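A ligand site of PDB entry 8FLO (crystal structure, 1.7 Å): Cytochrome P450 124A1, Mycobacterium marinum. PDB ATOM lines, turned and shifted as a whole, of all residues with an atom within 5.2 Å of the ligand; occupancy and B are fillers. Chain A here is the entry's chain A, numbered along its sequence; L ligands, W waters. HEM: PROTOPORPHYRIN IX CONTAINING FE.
Water W4 lies within hydrogen-bond range of an oxygen (O2A) of the ligand (2.6 Å), the guanidinium group of Arg 324 (2.8 Å) and the side-chain sulfur of Met 322 (3.3 Å).
Water W2 lies within hydrogen-bond range of an oxygen (O1A) of the ligand, the backbone carbonyl oxygen of Gly 378 and the backbone NH of His 381.
Water W3 lies within hydrogen-bond range of N of Gly 378, O1A of the ligand, O of Phe 375 and N of Gly 377.
Water W1 lies within hydrogen-bond range of the side-chain hydroxyl of Ser 86 (2.5 Å), the side-chain hydroxyl of Tyr 347 (2.8 Å), an oxygen (O1A) of the ligand (2.9 Å) and the backbone NH of Gly 377 (3.1 Å).
An iron atom (FE) of the ligand is bound by the side-chain sulfur (SG) of Cys 383, 2.3 Å away.
NH1 of Arg 126 lies within salt-bridge range of O1D of the ligand, at 2.7 Å.
A ring nitrogen (NE2) of His 122 is in hydrogen-bond range of an oxygen (O1D) of the ligand (2.6 Å).
A ring nitrogen (ND1) of His 381 is in hydrogen-bond range of an oxygen (O2D) of the ligand (2.8 Å).
NH2 of Arg 324 is in salt-bridge range of O2A of the ligand.
The side-chain sulfur of Cys 383 sits close to the backbone NH of Ala 386, at 3.3 Å.
NE2 of His 122 sits at hydrogen-bond distance from ND1 of His 381, 3.3 Å away.
The backbone carbonyl oxygen (O) of Ala 271 is in hydrogen-bond range of the side-chain hydroxyl (OG1) of Thr 275.
SG of Cys 383 sits close to N of Gly 385 (3.3 Å).
NH1 of Arg 126 lies within hydrogen-bond range of O of Ala 380 (3.4 Å).
The guanidinium group (NH1) of Arg 126 sits at hydrogen-bond distance from the backbone carbonyl oxygen (O) of Phe 382 (2.9 Å).
The side-chain carboxylate (OE2) of Glu 392 lies close to the side-chain hydroxyl (OG1) of Thr 276 (3.2 Å).
N of Cys 383 sits at hydrogen-bond distance from O of Phe 375.
SD of Met 114 lies close to O1D of the ligand, at 3.8 Å.
O of Ala 271 sits close to NC of the ligand.
CA of Ile 115 touches O2D of the ligand, 3.2 Å away.
Phe 264 touches the ligand.
Leu 267 touches the ligand (CD2 to CMD, 3.7 Å).
Leu 268 touches the ligand.
CA of Gly 272 touches C2C of the ligand, 3.4 Å away.
OG1 of Thr 275 touches C4B of the ligand, at 3.3 Å.
Thr 276 touches the ligand.
Ala 279 touches the ligand.
Pro 318 touches the ligand.
CG2 of Val 319 touches CHB of the ligand, 3.99 Å away.
Tyr 347 touches the ligand (CE2 to CMA, 3.8 Å).
Gly 374 touches the ligand.
O of Phe 375 touches CBA of the ligand, at 3.6 Å.
Gly 376 touches the ligand (N to CMA, 3.6 Å).
Ala 380 touches the ligand.
Leu 384 touches the ligand (CB to CMD, 3.6 Å).
CA of Gly 385 touches C3C of the ligand, 3.5 Å away.
CD2 of Leu 388 touches CBC of the ligand, at 3.7 Å.
Ala 389 touches the ligand (CB to CAB, 3.5 Å).
Glu 392 touches the ligand.
Hydrophobic or aromatic side chains within 4 Å of the ligand: Met 114, Ile 115, His 122, Phe 264, Leu 267, Leu 268, Ala 279, Pro 318, Val 319, Tyr 347, Phe 375, His 381, Leu 384, Leu 388 and Ala 389.
27 residues have an atom within 4 Å of the ligand: Met 114, Ile 115, His 122, Arg 126, Phe 264, Leu 267, Leu 268, Ala 271, Gly 272, Thr 275, Thr 276, Ala 279, Pro 318, Val 319, Arg 324, Tyr 347, Gly 374, Phe 375, Gly 376, Ala 380, His 381, Cys 383, Leu 384, Gly 385, Leu 388, Ala 389 and Glu 392.
The nearest printed residue that does not touch the ligand is Phe 382 (4.05 Å).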
ATOM      1  N   SER A  86      24.091   8.687  -4.438  1.00  0.00           N
ATOM      2  CA  SER A  86      23.400   9.794  -5.110  1.00  0.00           C
ATOM      3  C   SER A  86      22.865   9.401  -6.497  1.00  0.00           C
ATOM      4  O   SER A  86      21.816   9.914  -6.922  1.00  0.00           O
ATOM      5  CB  SER A  86      24.364  10.989  -5.200  1.00  0.00           C
ATOM      6  OG  SER A  86      24.888  11.332  -3.912  1.00  0.00           O
ATOM      7  N   MET A 114      10.621  19.963  -2.817  1.00  0.00           N
ATOM      8  CA  MET A 114      11.136  18.859  -3.637  1.00  0.00           C
ATOM      9  C   MET A 114      12.224  18.024  -2.974  1.00  0.00           C
ATOM     10  O   MET A 114      12.461  16.872  -3.400  1.00  0.00           O
ATOM     11  CB  MET A 114      11.657  19.385  -4.985  1.00  0.00           C
ATOM     12  CG  MET A 114      12.911  20.322  -4.847  1.00  0.00           C
ATOM     13  SD  MET A 114      13.359  20.963  -6.477  1.00  0.00           S
ATOM     14  CE  MET A 114      12.052  22.158  -6.779  1.00  0.00           C
ATOM     15  N   ILE A 115      12.933  18.542  -1.967  1.00  0.00           N
ATOM     16  CA  ILE A 115      14.086  17.777  -1.492  1.00  0.00           C
ATOM     17  C   ILE A 115      13.670  16.496  -0.738  1.00  0.00           C
ATOM     18  O   ILE A 115      14.493  15.588  -0.595  1.00  0.00           O
ATOM     19  CB  ILE A 115      15.003  18.710  -0.639  1.00  0.00           C
ATOM     20  CG1 ILE A 115      16.455  18.266  -0.681  1.00  0.00           C
ATOM     21  CG2 ILE A 115      14.538  18.826   0.829  1.00  0.00           C
ATOM     22  CD1 ILE A 115      17.422  19.366  -0.121  1.00  0.00           C
ATOM     23  N   HIS A 122       8.940  13.869  -7.360  1.00  0.00           N
ATOM     24  CA  HIS A 122      10.060  14.799  -7.357  1.00  0.00           C
ATOM     25  C   HIS A 122      10.293  15.379  -8.742  1.00  0.00           C
ATOM     26  O   HIS A 122      10.410  16.613  -8.891  1.00  0.00           O
ATOM     27  CB  HIS A 122      11.343  14.097  -6.887  1.00  0.00           C
ATOM     28  CG  HIS A 122      12.583  14.920  -7.118  1.00  0.00           C
ATOM     29  ND1 HIS A 122      13.447  14.705  -8.165  1.00  0.00           N
ATOM     30  CD2 HIS A 122      13.063  15.995  -6.450  1.00  0.00           C
ATOM     31  CE1 HIS A 122      14.436  15.580  -8.107  1.00  0.00           C
ATOM     32  NE2 HIS A 122      14.230  16.370  -7.076  1.00  0.00           N
ATOM     33  N   ARG A 126      10.100  19.389  -9.707  1.00  0.00           N
ATOM     34  CA  ARG A 126      11.328  20.082 -10.086  1.00  0.00           C
ATOM     35  C   ARG A 126      11.271  20.561 -11.531  1.00  0.00           C
ATOM     36  O   ARG A 126      11.818  21.635 -11.832  1.00  0.00           O
ATOM     37  CB  ARG A 126      12.520  19.169  -9.883  1.00  0.00           C
ATOM     38  CG  ARG A 126      13.822  19.833 -10.267  1.00  0.00           C
ATOM     39  CD  ARG A 126      15.075  19.068  -9.745  1.00  0.00           C
ATOM     40  NE  ARG A 126      16.327  19.631 -10.293  1.00  0.00           N
ATOM     41  CZ  ARG A 126      17.485  19.634  -9.629  1.00  0.00           C
ATOM     42  NH1 ARG A 126      17.549  19.144  -8.380  1.00  0.00           N
ATOM     43  NH2 ARG A 126      18.570  20.167 -10.179  1.00  0.00           N
ATOM     44  N   ILE A 180      17.088  36.111  -2.429  1.00  0.00           N
ATOM     45  CA  ILE A 180      15.834  35.347  -2.507  1.00  0.00           C
ATOM     46  C   ILE A 180      14.613  36.288  -2.491  1.00  0.00           C
ATOM     47  O   ILE A 180      13.679  36.129  -3.281  1.00  0.00           O
ATOM     48  CB  ILE A 180      15.775  34.335  -1.349  1.00  0.00           C
ATOM     49  CG1 ILE A 180      16.784  33.207  -1.582  1.00  0.00           C
ATOM     50  CG2 ILE A 180      14.300  33.800  -1.236  1.00  0.00           C
ATOM     51  CD1 ILE A 180      17.051  32.383  -0.383  1.00  0.00           C
ATOM     52  N   MET A 183      14.237  37.858  -5.927  1.00  0.00           N
ATOM     53  CA  MET A 183      13.650  37.044  -7.006  1.00  0.00           C
ATOM     54  C   MET A 183      12.161  36.780  -6.805  1.00  0.00           C
ATOM     55  O   MET A 183      11.398  36.688  -7.790  1.00  0.00           O
ATOM     56  CB  MET A 183      14.351  35.682  -7.212  1.00  0.00           C
ATOM     57  CG  MET A 183      14.269  34.687  -6.064  1.00  0.00           C
ATOM     58  SD  MET A 183      15.182  33.141  -6.484  1.00  0.00           S
ATOM     59  CE  MET A 183      16.817  33.832  -6.311  1.00  0.00           C
ATOM     60  N   PHE A 264       7.976  25.606  -1.527  1.00  0.00           N
ATOM     61  CA  PHE A 264       9.247  25.823  -2.216  1.00  0.00           C
ATOM     62  C   PHE A 264       9.924  27.086  -1.713  1.00  0.00           C
ATOM     63  O   PHE A 264      11.150  27.110  -1.493  1.00  0.00           O
ATOM     64  CB  PHE A 264       9.015  25.909  -3.740  1.00  0.00           C
ATOM     65  CG  PHE A 264      10.283  26.254  -4.537  1.00  0.00           C
ATOM     66  CD1 PHE A 264      11.344  25.368  -4.609  1.00  0.00           C
ATOM     67  CD2 PHE A 264      10.391  27.483  -5.187  1.00  0.00           C
ATOM     68  CE1 PHE A 264      12.494  25.691  -5.321  1.00  0.00           C
ATOM     69  CE2 PHE A 264      11.547  27.804  -5.920  1.00  0.00           C
ATOM     70  CZ  PHE A 264      12.588  26.910  -5.988  1.00  0.00           C
ATOM     71  N   LEU A 267      11.552  26.191   1.544  1.00  0.00           N
ATOM     72  CA  LEU A 267      12.796  25.495   1.284  1.00  0.00           C
ATOM     73  C   LEU A 267      13.890  26.464   0.876  1.00  0.00           C
ATOM     74  O   LEU A 267      15.020  26.369   1.364  1.00  0.00           O
ATOM     75  CB  LEU A 267      12.577  24.426   0.221  1.00  0.00           C
ATOM     76  CG  LEU A 267      13.851  23.710  -0.307  1.00  0.00           C
ATOM     77  CD1 LEU A 267      14.485  22.812   0.762  1.00  0.00           C
ATOM     78  CD2 LEU A 267      13.562  22.971  -1.682  1.00  0.00           C
ATOM     79  N   LEU A 268      13.577  27.447   0.021  1.00  0.00           N
ATOM     80  CA  LEU A 268      14.638  28.380  -0.405  1.00  0.00           C
ATOM     81  C   LEU A 268      15.233  29.177   0.751  1.00  0.00           C
ATOM     82  O   LEU A 268      16.449  29.405   0.792  1.00  0.00           O
ATOM     83  CB  LEU A 268      14.146  29.369  -1.458  1.00  0.00           C
ATOM     84  CG  LEU A 268      13.865  28.982  -2.906  1.00  0.00           C
ATOM     85  CD1 LEU A 268      13.440  30.211  -3.742  1.00  0.00           C
ATOM     86  CD2 LEU A 268      14.957  28.214  -3.571  1.00  0.00           C
ATOM     87  N   ALA A 271      17.500  26.181   2.547  1.00  0.00           N
ATOM     88  CA  ALA A 271      18.479  25.502   1.711  1.00  0.00           C
ATOM     89  C   ALA A 271      19.262  26.418   0.771  1.00  0.00           C
ATOM     90  O   ALA A 271      20.425  26.127   0.431  1.00  0.00           O
ATOM     91  CB  ALA A 271      17.831  24.398   0.918  1.00  0.00           C
ATOM     92  N   GLY A 272      18.678  27.528   0.324  1.00  0.00           N
ATOM     93  CA  GLY A 272      19.362  28.455  -0.546  1.00  0.00           C
ATOM     94  C   GLY A 272      19.961  29.639   0.161  1.00  0.00           C
ATOM     95  O   GLY A 272      20.424  30.585  -0.493  1.00  0.00           O
ATOM     96  N   THR A 275      23.223  27.885   3.609  1.00  0.00           N
ATOM     97  CA  THR A 275      24.306  27.239   2.872  1.00  0.00           C
ATOM     98  C   THR A 275      25.251  28.283   2.288  1.00  0.00           C
ATOM     99  O   THR A 275      26.473  28.276   2.556  1.00  0.00           O
ATOM    100  CB  THR A 275      23.737  26.379   1.760  1.00  0.00           C
ATOM    101  OG1 THR A 275      22.882  27.214   0.949  1.00  0.00           O
ATOM    102  CG2 THR A 275      22.857  25.229   2.310  1.00  0.00           C
ATOM    103  N   THR A 276      24.702  29.196   1.459  1.00  0.00           N
ATOM    104  CA  THR A 276      25.564  30.215   0.839  1.00  0.00           C
ATOM    105  C   THR A 276      26.267  31.082   1.896  1.00  0.00           C
ATOM    106  O   THR A 276      27.428  31.464   1.714  1.00  0.00           O
ATOM    107  CB  THR A 276      24.735  31.079  -0.109  1.00  0.00           C
ATOM    108  OG1 THR A 276      24.137  30.233  -1.061  1.00  0.00           O
ATOM    109  CG2 THR A 276      25.613  32.072  -0.816  1.00  0.00           C
ATOM    110  N   ALA A 279      29.261  29.211   3.116  1.00  0.00           N
ATOM    111  CA  ALA A 279      30.315  29.198   2.110  1.00  0.00           C
ATOM    112  C   ALA A 279      31.092  30.511   2.111  1.00  0.00           C
ATOM    113  O   ALA A 279      32.339  30.528   1.978  1.00  0.00           O
ATOM    114  CB  ALA A 279      29.701  28.898   0.730  1.00  0.00           C
ATOM    115  N   VAL A 313      33.827  26.038  -2.077  1.00  0.00           N
ATOM    116  CA  VAL A 313      32.783  25.069  -1.756  1.00  0.00           C
ATOM    117  C   VAL A 313      33.355  23.751  -1.251  1.00  0.00           C
ATOM    118  O   VAL A 313      32.822  23.173  -0.291  1.00  0.00           O
ATOM    119  CB  VAL A 313      31.851  24.863  -2.959  1.00  0.00           C
ATOM    120  CG1 VAL A 313      30.794  23.780  -2.660  1.00  0.00           C
ATOM    121  CG2 VAL A 313      31.222  26.186  -3.256  1.00  0.00           C
ATOM    122  N   PRO A 318      29.411  23.418   3.099  1.00  0.00           N
ATOM    123  CA  PRO A 318      28.397  24.018   4.005  1.00  0.00           C
ATOM    124  C   PRO A 318      27.347  23.038   4.477  1.00  0.00           C
ATOM    125  O   PRO A 318      26.925  23.133   5.643  1.00  0.00           O
ATOM    126  CB  PRO A 318      27.809  25.157   3.142  1.00  0.00           C
ATOM    127  CG  PRO A 318      28.926  25.515   2.188  1.00  0.00           C
ATOM    128  CD  PRO A 318      29.594  24.205   1.867  1.00  0.00           C
ATOM    129  N   VAL A 319      26.897  22.119   3.610  1.00  0.00           N
ATOM    130  CA  VAL A 319      26.057  20.990   4.006  1.00  0.00           C
ATOM    131  C   VAL A 319      26.957  19.831   4.366  1.00  0.00           C
ATOM    132  O   VAL A 319      27.676  19.288   3.510  1.00  0.00           O
ATOM    133  CB  VAL A 319      25.097  20.600   2.883  1.00  0.00           C
ATOM    134  CG1 VAL A 319      24.339  19.333   3.305  1.00  0.00           C
ATOM    135  CG2 VAL A 319      24.142  21.754   2.680  1.00  0.00           C
ATOM    136  N   MET A 322      23.764  14.608   4.040  1.00  0.00           N
ATOM    137  CA  MET A 322      22.353  14.404   3.712  1.00  0.00           C
ATOM    138  C   MET A 322      22.014  12.934   3.993  1.00  0.00           C
ATOM    139  O   MET A 322      22.855  12.048   3.814  1.00  0.00           O
ATOM    140  CB  MET A 322      22.128  14.765   2.197  1.00  0.00           C
ATOM    141  CG  MET A 322      21.946  16.272   1.802  1.00  0.00           C
ATOM    142  SD  MET A 322      20.360  17.000   2.436  1.00  0.00           S
ATOM    143  CE  MET A 322      20.541  18.767   2.249  1.00  0.00           C
ATOM    144  N   ARG A 324      19.527   9.494   3.557  1.00  0.00           N
ATOM    145  CA  ARG A 324      18.735   8.687   2.667  1.00  0.00           C
ATOM    146  C   ARG A 324      18.132   7.545   3.491  1.00  0.00           C
ATOM    147  O   ARG A 324      18.524   7.295   4.644  1.00  0.00           O
ATOM    148  CB  ARG A 324      19.628   8.184   1.530  1.00  0.00           C
ATOM    149  CG  ARG A 324      20.164   9.280   0.592  1.00  0.00           C
ATOM    150  CD  ARG A 324      19.062   9.914  -0.217  1.00  0.00           C
ATOM    151  NE  ARG A 324      19.515  10.787  -1.304  1.00  0.00           N
ATOM    152  CZ  ARG A 324      19.747  12.093  -1.183  1.00  0.00           C
ATOM    153  NH1 ARG A 324      19.577  12.698  -0.004  1.00  0.00           N
ATOM    154  NH2 ARG A 324      20.070  12.819  -2.258  1.00  0.00           N
ATOM    155  N   TYR A 347      29.409  14.659   3.003  1.00  0.00           N
ATOM    156  CA  TYR A 347      30.137  15.461   1.984  1.00  0.00           C
ATOM    157  C   TYR A 347      31.421  16.037   2.603  1.00  0.00           C
ATOM    158  O   TYR A 347      32.409  16.152   1.865  1.00  0.00           O
ATOM    159  CB  TYR A 347      29.240  16.582   1.454  1.00  0.00           C
ATOM    160  CG  TYR A 347      27.907  16.095   0.957  1.00  0.00           C
ATOM    161  CD1 TYR A 347      27.821  15.053   0.041  1.00  0.00           C
ATOM    162  CD2 TYR A 347      26.729  16.667   1.403  1.00  0.00           C
ATOM    163  CE1 TYR A 347      26.592  14.598  -0.424  1.00  0.00           C
ATOM    164  CE2 TYR A 347      25.500  16.216   0.948  1.00  0.00           C
ATOM    165  CZ  TYR A 347      25.434  15.187   0.037  1.00  0.00           C
ATOM    166  OH  TYR A 347      24.226  14.744  -0.421  1.00  0.00           O
ATOM    167  N   GLY A 374      30.232  19.223  -2.611  1.00  0.00           N
ATOM    168  CA  GLY A 374      29.536  20.105  -1.665  1.00  0.00           C
ATOM    169  C   GLY A 374      28.119  20.441  -2.070  1.00  0.00           C
ATOM    170  O   GLY A 374      27.298  20.730  -1.214  1.00  0.00           O
ATOM    171  N   PHE A 375      27.799  20.387  -3.383  1.00  0.00           N
ATOM    172  CA  PHE A 375      26.425  20.510  -3.871  1.00  0.00           C
ATOM    173  C   PHE A 375      25.751  19.142  -3.998  1.00  0.00           C
ATOM    174  O   PHE A 375      24.714  19.034  -4.639  1.00  0.00           O
ATOM    175  CB  PHE A 375      26.437  21.211  -5.233  1.00  0.00           C
ATOM    176  CG  PHE A 375      26.929  22.642  -5.188  1.00  0.00           C
ATOM    177  CD1 PHE A 375      26.262  23.594  -4.443  1.00  0.00           C
ATOM    178  CD2 PHE A 375      28.031  23.034  -5.914  1.00  0.00           C
ATOM    179  CE1 PHE A 375      26.692  24.912  -4.456  1.00  0.00           C
ATOM    180  CE2 PHE A 375      28.482  24.347  -5.923  1.00  0.00           C
ATOM    181  CZ  PHE A 375      27.831  25.279  -5.190  1.00  0.00           C
ATOM    182  N   GLY A 376      26.329  18.117  -3.381  1.00  0.00           N
ATOM    183  CA  GLY A 376      25.882  16.746  -3.455  1.00  0.00           C
ATOM    184  C   GLY A 376      26.719  15.957  -4.442  1.00  0.00           C
ATOM    185  O   GLY A 376      27.597  16.490  -5.133  1.00  0.00           O
ATOM    186  N   GLY A 377      26.437  14.651  -4.475  1.00  0.00           N
ATOM    187  CA  GLY A 377      27.205  13.673  -5.259  1.00  0.00           C
ATOM    188  C   GLY A 377      26.781  13.580  -6.712  1.00  0.00           C
ATOM    189  O   GLY A 377      27.333  12.824  -7.524  1.00  0.00           O
ATOM    190  N   GLY A 378      25.809  14.391  -7.092  1.00  0.00           N
ATOM    191  CA  GLY A 378      25.270  14.326  -8.440  1.00  0.00           C
ATOM    192  C   GLY A 378      23.929  13.594  -8.504  1.00  0.00           C
ATOM    193  O   GLY A 378      23.456  12.978  -7.534  1.00  0.00           O
ATOM    194  N   ALA A 380      19.716  13.104  -9.277  1.00  0.00           N
ATOM    195  CA  ALA A 380      18.368  13.656  -9.385  1.00  0.00           C
ATOM    196  C   ALA A 380      18.126  14.898  -8.523  1.00  0.00           C
ATOM    197  O   ALA A 380      17.307  15.747  -8.883  1.00  0.00           O
ATOM    198  CB  ALA A 380      17.346  12.584  -8.990  1.00  0.00           C
ATOM    199  N   HIS A 381      18.763  14.971  -7.365  1.00  0.00           N
ATOM    200  CA  HIS A 381      18.563  16.046  -6.398  1.00  0.00           C
ATOM    201  C   HIS A 381      19.720  17.039  -6.402  1.00  0.00           C
ATOM    202  O   HIS A 381      19.816  17.856  -5.475  1.00  0.00           O
ATOM    203  CB  HIS A 381      18.358  15.460  -4.998  1.00  0.00           C
ATOM    204  CG  HIS A 381      17.053  14.738  -4.808  1.00  0.00           C
ATOM    205  ND1 HIS A 381      15.892  15.377  -4.406  1.00  0.00           N
ATOM    206  CD2 HIS A 381      16.736  13.426  -4.895  1.00  0.00           C
ATOM    207  CE1 HIS A 381      14.904  14.488  -4.301  1.00  0.00           C
ATOM    208  NE2 HIS A 381      15.400  13.291  -4.573  1.00  0.00           N
ATOM    209  N   PHE A 382      20.616  16.964  -7.395  1.00  0.00           N
ATOM    210  CA  PHE A 382      21.765  17.869  -7.446  1.00  0.00           C
ATOM    211  C   PHE A 382      21.321  19.313  -7.228  1.00  0.00           C
ATOM    212  O   PHE A 382      20.355  19.762  -7.841  1.00  0.00           O
ATOM    213  CB  PHE A 382      22.521  17.755  -8.782  1.00  0.00           C
ATOM    214  CG  PHE A 382      23.671  18.735  -8.859  1.00  0.00           C
ATOM    215  CD1 PHE A 382      24.873  18.456  -8.210  1.00  0.00           C
ATOM    216  CD2 PHE A 382      23.539  19.954  -9.523  1.00  0.00           C
ATOM    217  CE1 PHE A 382      25.923  19.367  -8.234  1.00  0.00           C
ATOM    218  CE2 PHE A 382      24.618  20.862  -9.556  1.00  0.00           C
ATOM    219  CZ  PHE A 382      25.778  20.563  -8.910  1.00  0.00           C
ATOM    220  N   CYS A 383      22.047  20.054  -6.364  1.00  0.00           N
ATOM    221  CA  CYS A 383      21.577  21.378  -5.919  1.00  0.00           C
ATOM    222  C   CYS A 383      20.963  22.195  -7.060  1.00  0.00           C
ATOM    223  O   CYS A 383      21.664  22.540  -8.021  1.00  0.00           O
ATOM    224  CB  CYS A 383      22.752  22.170  -5.311  1.00  0.00           C
ATOM    225  SG  CYS A 383      22.314  23.910  -4.881  1.00  0.00           S
ATOM    226  N   LEU A 384      19.666  22.566  -6.920  1.00  0.00           N
ATOM    227  CA  LEU A 384      19.038  23.383  -7.960  1.00  0.00           C
ATOM    228  C   LEU A 384      19.712  24.751  -8.089  1.00  0.00           C
ATOM    229  O   LEU A 384      19.755  25.324  -9.187  1.00  0.00           O
ATOM    230  CB  LEU A 384      17.519  23.601  -7.663  1.00  0.00           C
ATOM    231  CG  LEU A 384      16.673  24.307  -8.734  1.00  0.00           C
ATOM    232  CD1 LEU A 384      16.513  23.378  -9.875  1.00  0.00           C
ATOM    233  CD2 LEU A 384      15.315  24.742  -8.170  1.00  0.00           C
ATOM    234  N   GLY A 385      20.190  25.313  -6.989  1.00  0.00           N
ATOM    235  CA  GLY A 385      20.827  26.605  -7.104  1.00  0.00           C
ATOM    236  C   GLY A 385      22.344  26.613  -7.201  1.00  0.00           C
ATOM    237  O   GLY A 385      22.911  27.645  -6.889  1.00  0.00           O
ATOM    238  N   ALA A 386      23.014  25.537  -7.672  1.00  0.00           N
ATOM    239  CA  ALA A 386      24.472  25.501  -7.548  1.00  0.00           C
ATOM    240  C   ALA A 386      25.124  26.659  -8.300  1.00  0.00           C
ATOM    241  O   ALA A 386      26.080  27.241  -7.808  1.00  0.00           O
ATOM    242  CB  ALA A 386      25.034  24.167  -8.074  1.00  0.00           C
ATOM    243  N   LEU A 388      23.776  29.546  -9.062  1.00  0.00           N
ATOM    244  CA  LEU A 388      23.443  30.780  -8.345  1.00  0.00           C
ATOM    245  C   LEU A 388      24.386  30.928  -7.147  1.00  0.00           C
ATOM    246  O   LEU A 388      24.970  32.009  -6.947  1.00  0.00           O
ATOM    247  CB  LEU A 388      21.961  30.787  -7.919  1.00  0.00           C
ATOM    248  CG  LEU A 388      21.561  31.968  -7.011  1.00  0.00           C
ATOM    249  CD1 LEU A 388      21.956  33.341  -7.577  1.00  0.00           C
ATOM    250  CD2 LEU A 388      20.066  31.974  -6.585  1.00  0.00           C
ATOM    251  N   ALA A 389      24.644  29.826  -6.413  1.00  0.00           N
ATOM    252  CA  ALA A 389      25.564  29.916  -5.265  1.00  0.00           C
ATOM    253  C   ALA A 389      26.980  30.295  -5.716  1.00  0.00           C
ATOM    254  O   ALA A 389      27.614  31.192  -5.145  1.00  0.00           O
ATOM    255  CB  ALA A 389      25.584  28.599  -4.478  1.00  0.00           C
ATOM    256  N   GLU A 392      26.979  34.027  -6.314  1.00  0.00           N
ATOM    257  CA  GLU A 392      26.980  34.814  -5.085  1.00  0.00           C
ATOM    258  C   GLU A 392      28.364  34.821  -4.449  1.00  0.00           C
ATOM    259  O   GLU A 392      28.830  35.881  -4.031  1.00  0.00           O
ATOM    260  CB  GLU A 392      25.959  34.302  -4.074  1.00  0.00           C
ATOM    261  CG  GLU A 392      24.459  34.414  -4.628  1.00  0.00           C
ATOM    262  CD  GLU A 392      23.430  33.543  -3.875  1.00  0.00           C
ATOM    263  OE1 GLU A 392      22.233  33.894  -3.822  1.00  0.00           O
ATOM    264  OE2 GLU A 392      23.805  32.482  -3.314  1.00  0.00           O
ATOM    265  N   ILE A 393      29.015  33.656  -4.363  1.00  0.00           N
ATOM    266  CA  ILE A 393      30.370  33.588  -3.825  1.00  0.00           C
ATOM    267  C   ILE A 393      31.321  34.462  -4.638  1.00  0.00           C
ATOM    268  O   ILE A 393      32.114  35.237  -4.068  1.00  0.00           O
ATOM    269  CB  ILE A 393      30.845  32.136  -3.748  1.00  0.00           C
ATOM    270  CG1 ILE A 393      29.933  31.318  -2.827  1.00  0.00           C
ATOM    271  CG2 ILE A 393      32.275  32.105  -3.226  1.00  0.00           C
ATOM    272  CD1 ILE A 393      30.057  29.788  -3.104  1.00  0.00           C
HETATM  273  CHA HEM L   1      19.667  20.825  -2.988  1.00  0.00           C
HETATM  274  CHB HEM L   1      23.987  22.273  -1.278  1.00  0.00           C
HETATM  275  CHC HEM L   1      22.928  26.917  -2.375  1.00  0.00           C
HETATM  276  CHD HEM L   1      18.451  25.492  -3.822  1.00  0.00           C
HETATM  277  C1A HEM L   1      20.926  20.800  -2.396  1.00  0.00           C
HETATM  278  C2A HEM L   1      21.664  19.638  -1.906  1.00  0.00           C
HETATM  279  C3A HEM L   1      22.837  20.080  -1.459  1.00  0.00           C
HETATM  280  C4A HEM L   1      22.903  21.512  -1.631  1.00  0.00           C
HETATM  281  CMA HEM L   1      23.969  19.231  -0.832  1.00  0.00           C
HETATM  282  CAA HEM L   1      21.211  18.156  -1.914  1.00  0.00           C
HETATM  283  CBA HEM L   1      21.930  17.427  -3.080  1.00  0.00           C
HETATM  284  CGA HEM L   1      21.598  15.939  -3.169  1.00  0.00           C
HETATM  285  O1A HEM L   1      22.173  15.246  -4.079  1.00  0.00           O
HETATM  286  O2A HEM L   1      20.828  15.389  -2.321  1.00  0.00           O
HETATM  287  C1B HEM L   1      24.086  23.645  -1.418  1.00  0.00           C
HETATM  288  C2B HEM L   1      25.223  24.456  -1.099  1.00  0.00           C
HETATM  289  C3B HEM L   1      24.931  25.729  -1.405  1.00  0.00           C
HETATM  290  C4B HEM L   1      23.592  25.777  -1.955  1.00  0.00           C
HETATM  291  CMB HEM L   1      26.553  23.881  -0.478  1.00  0.00           C
HETATM  292  CAB HEM L   1      25.767  27.033  -1.307  1.00  0.00           C
HETATM  293  CBB HEM L   1      27.118  27.081  -1.217  1.00  0.00           C
HETATM  294  C1C HEM L   1      21.662  26.931  -2.939  1.00  0.00           C
HETATM  295  C2C HEM L   1      20.967  28.096  -3.495  1.00  0.00           C
HETATM  296  C3C HEM L   1      19.743  27.670  -3.918  1.00  0.00           C
HETATM  297  C4C HEM L   1      19.598  26.258  -3.581  1.00  0.00           C
HETATM  298  CMC HEM L   1      21.624  29.501  -3.610  1.00  0.00           C
HETATM  299  CAC HEM L   1      18.626  28.511  -4.563  1.00  0.00           C
HETATM  300  CBC HEM L   1      18.375  29.758  -4.117  1.00  0.00           C
HETATM  301  C1D HEM L   1      18.353  24.112  -3.700  1.00  0.00           C
HETATM  302  C2D HEM L   1      17.176  23.268  -4.015  1.00  0.00           C
HETATM  303  C3D HEM L   1      17.531  21.987  -3.782  1.00  0.00           C
HETATM  304  C4D HEM L   1      18.931  21.974  -3.314  1.00  0.00           C
HETATM  305  CMD HEM L   1      15.777  23.811  -4.466  1.00  0.00           C
HETATM  306  CAD HEM L   1      16.664  20.720  -3.898  1.00  0.00           C
HETATM  307  CBD HEM L   1      16.910  20.040  -5.239  1.00  0.00           C
HETATM  308  CGD HEM L   1      16.177  18.703  -5.261  1.00  0.00           C
HETATM  309  O1D HEM L   1      15.949  18.207  -6.397  1.00  0.00           O
HETATM  310  O2D HEM L   1      15.785  18.138  -4.202  1.00  0.00           O
HETATM  311  NA  HEM L   1      21.736  21.897  -2.263  1.00  0.00           N
HETATM  312  NB  HEM L   1      23.103  24.493  -1.894  1.00  0.00           N
HETATM  313  NC  HEM L   1      20.810  25.846  -2.978  1.00  0.00           N
HETATM  314  ND  HEM L   1      19.375  23.290  -3.303  1.00  0.00           N
HETATM  315 FE   HEM L   1      21.347  23.860  -2.791  1.00  0.00          FE
HETATM  316  O   HOH W   1      24.108  13.489  -2.874  1.00  0.00           O
HETATM  317  O   HOH W   2      21.197  13.387  -5.860  1.00  0.00           O
HETATM  318  O   HOH W   3      24.042  16.298  -5.954  1.00  0.00           O
HETATM  319  O   HOH W   4      19.287  15.433  -0.207  1.00  0.00           O
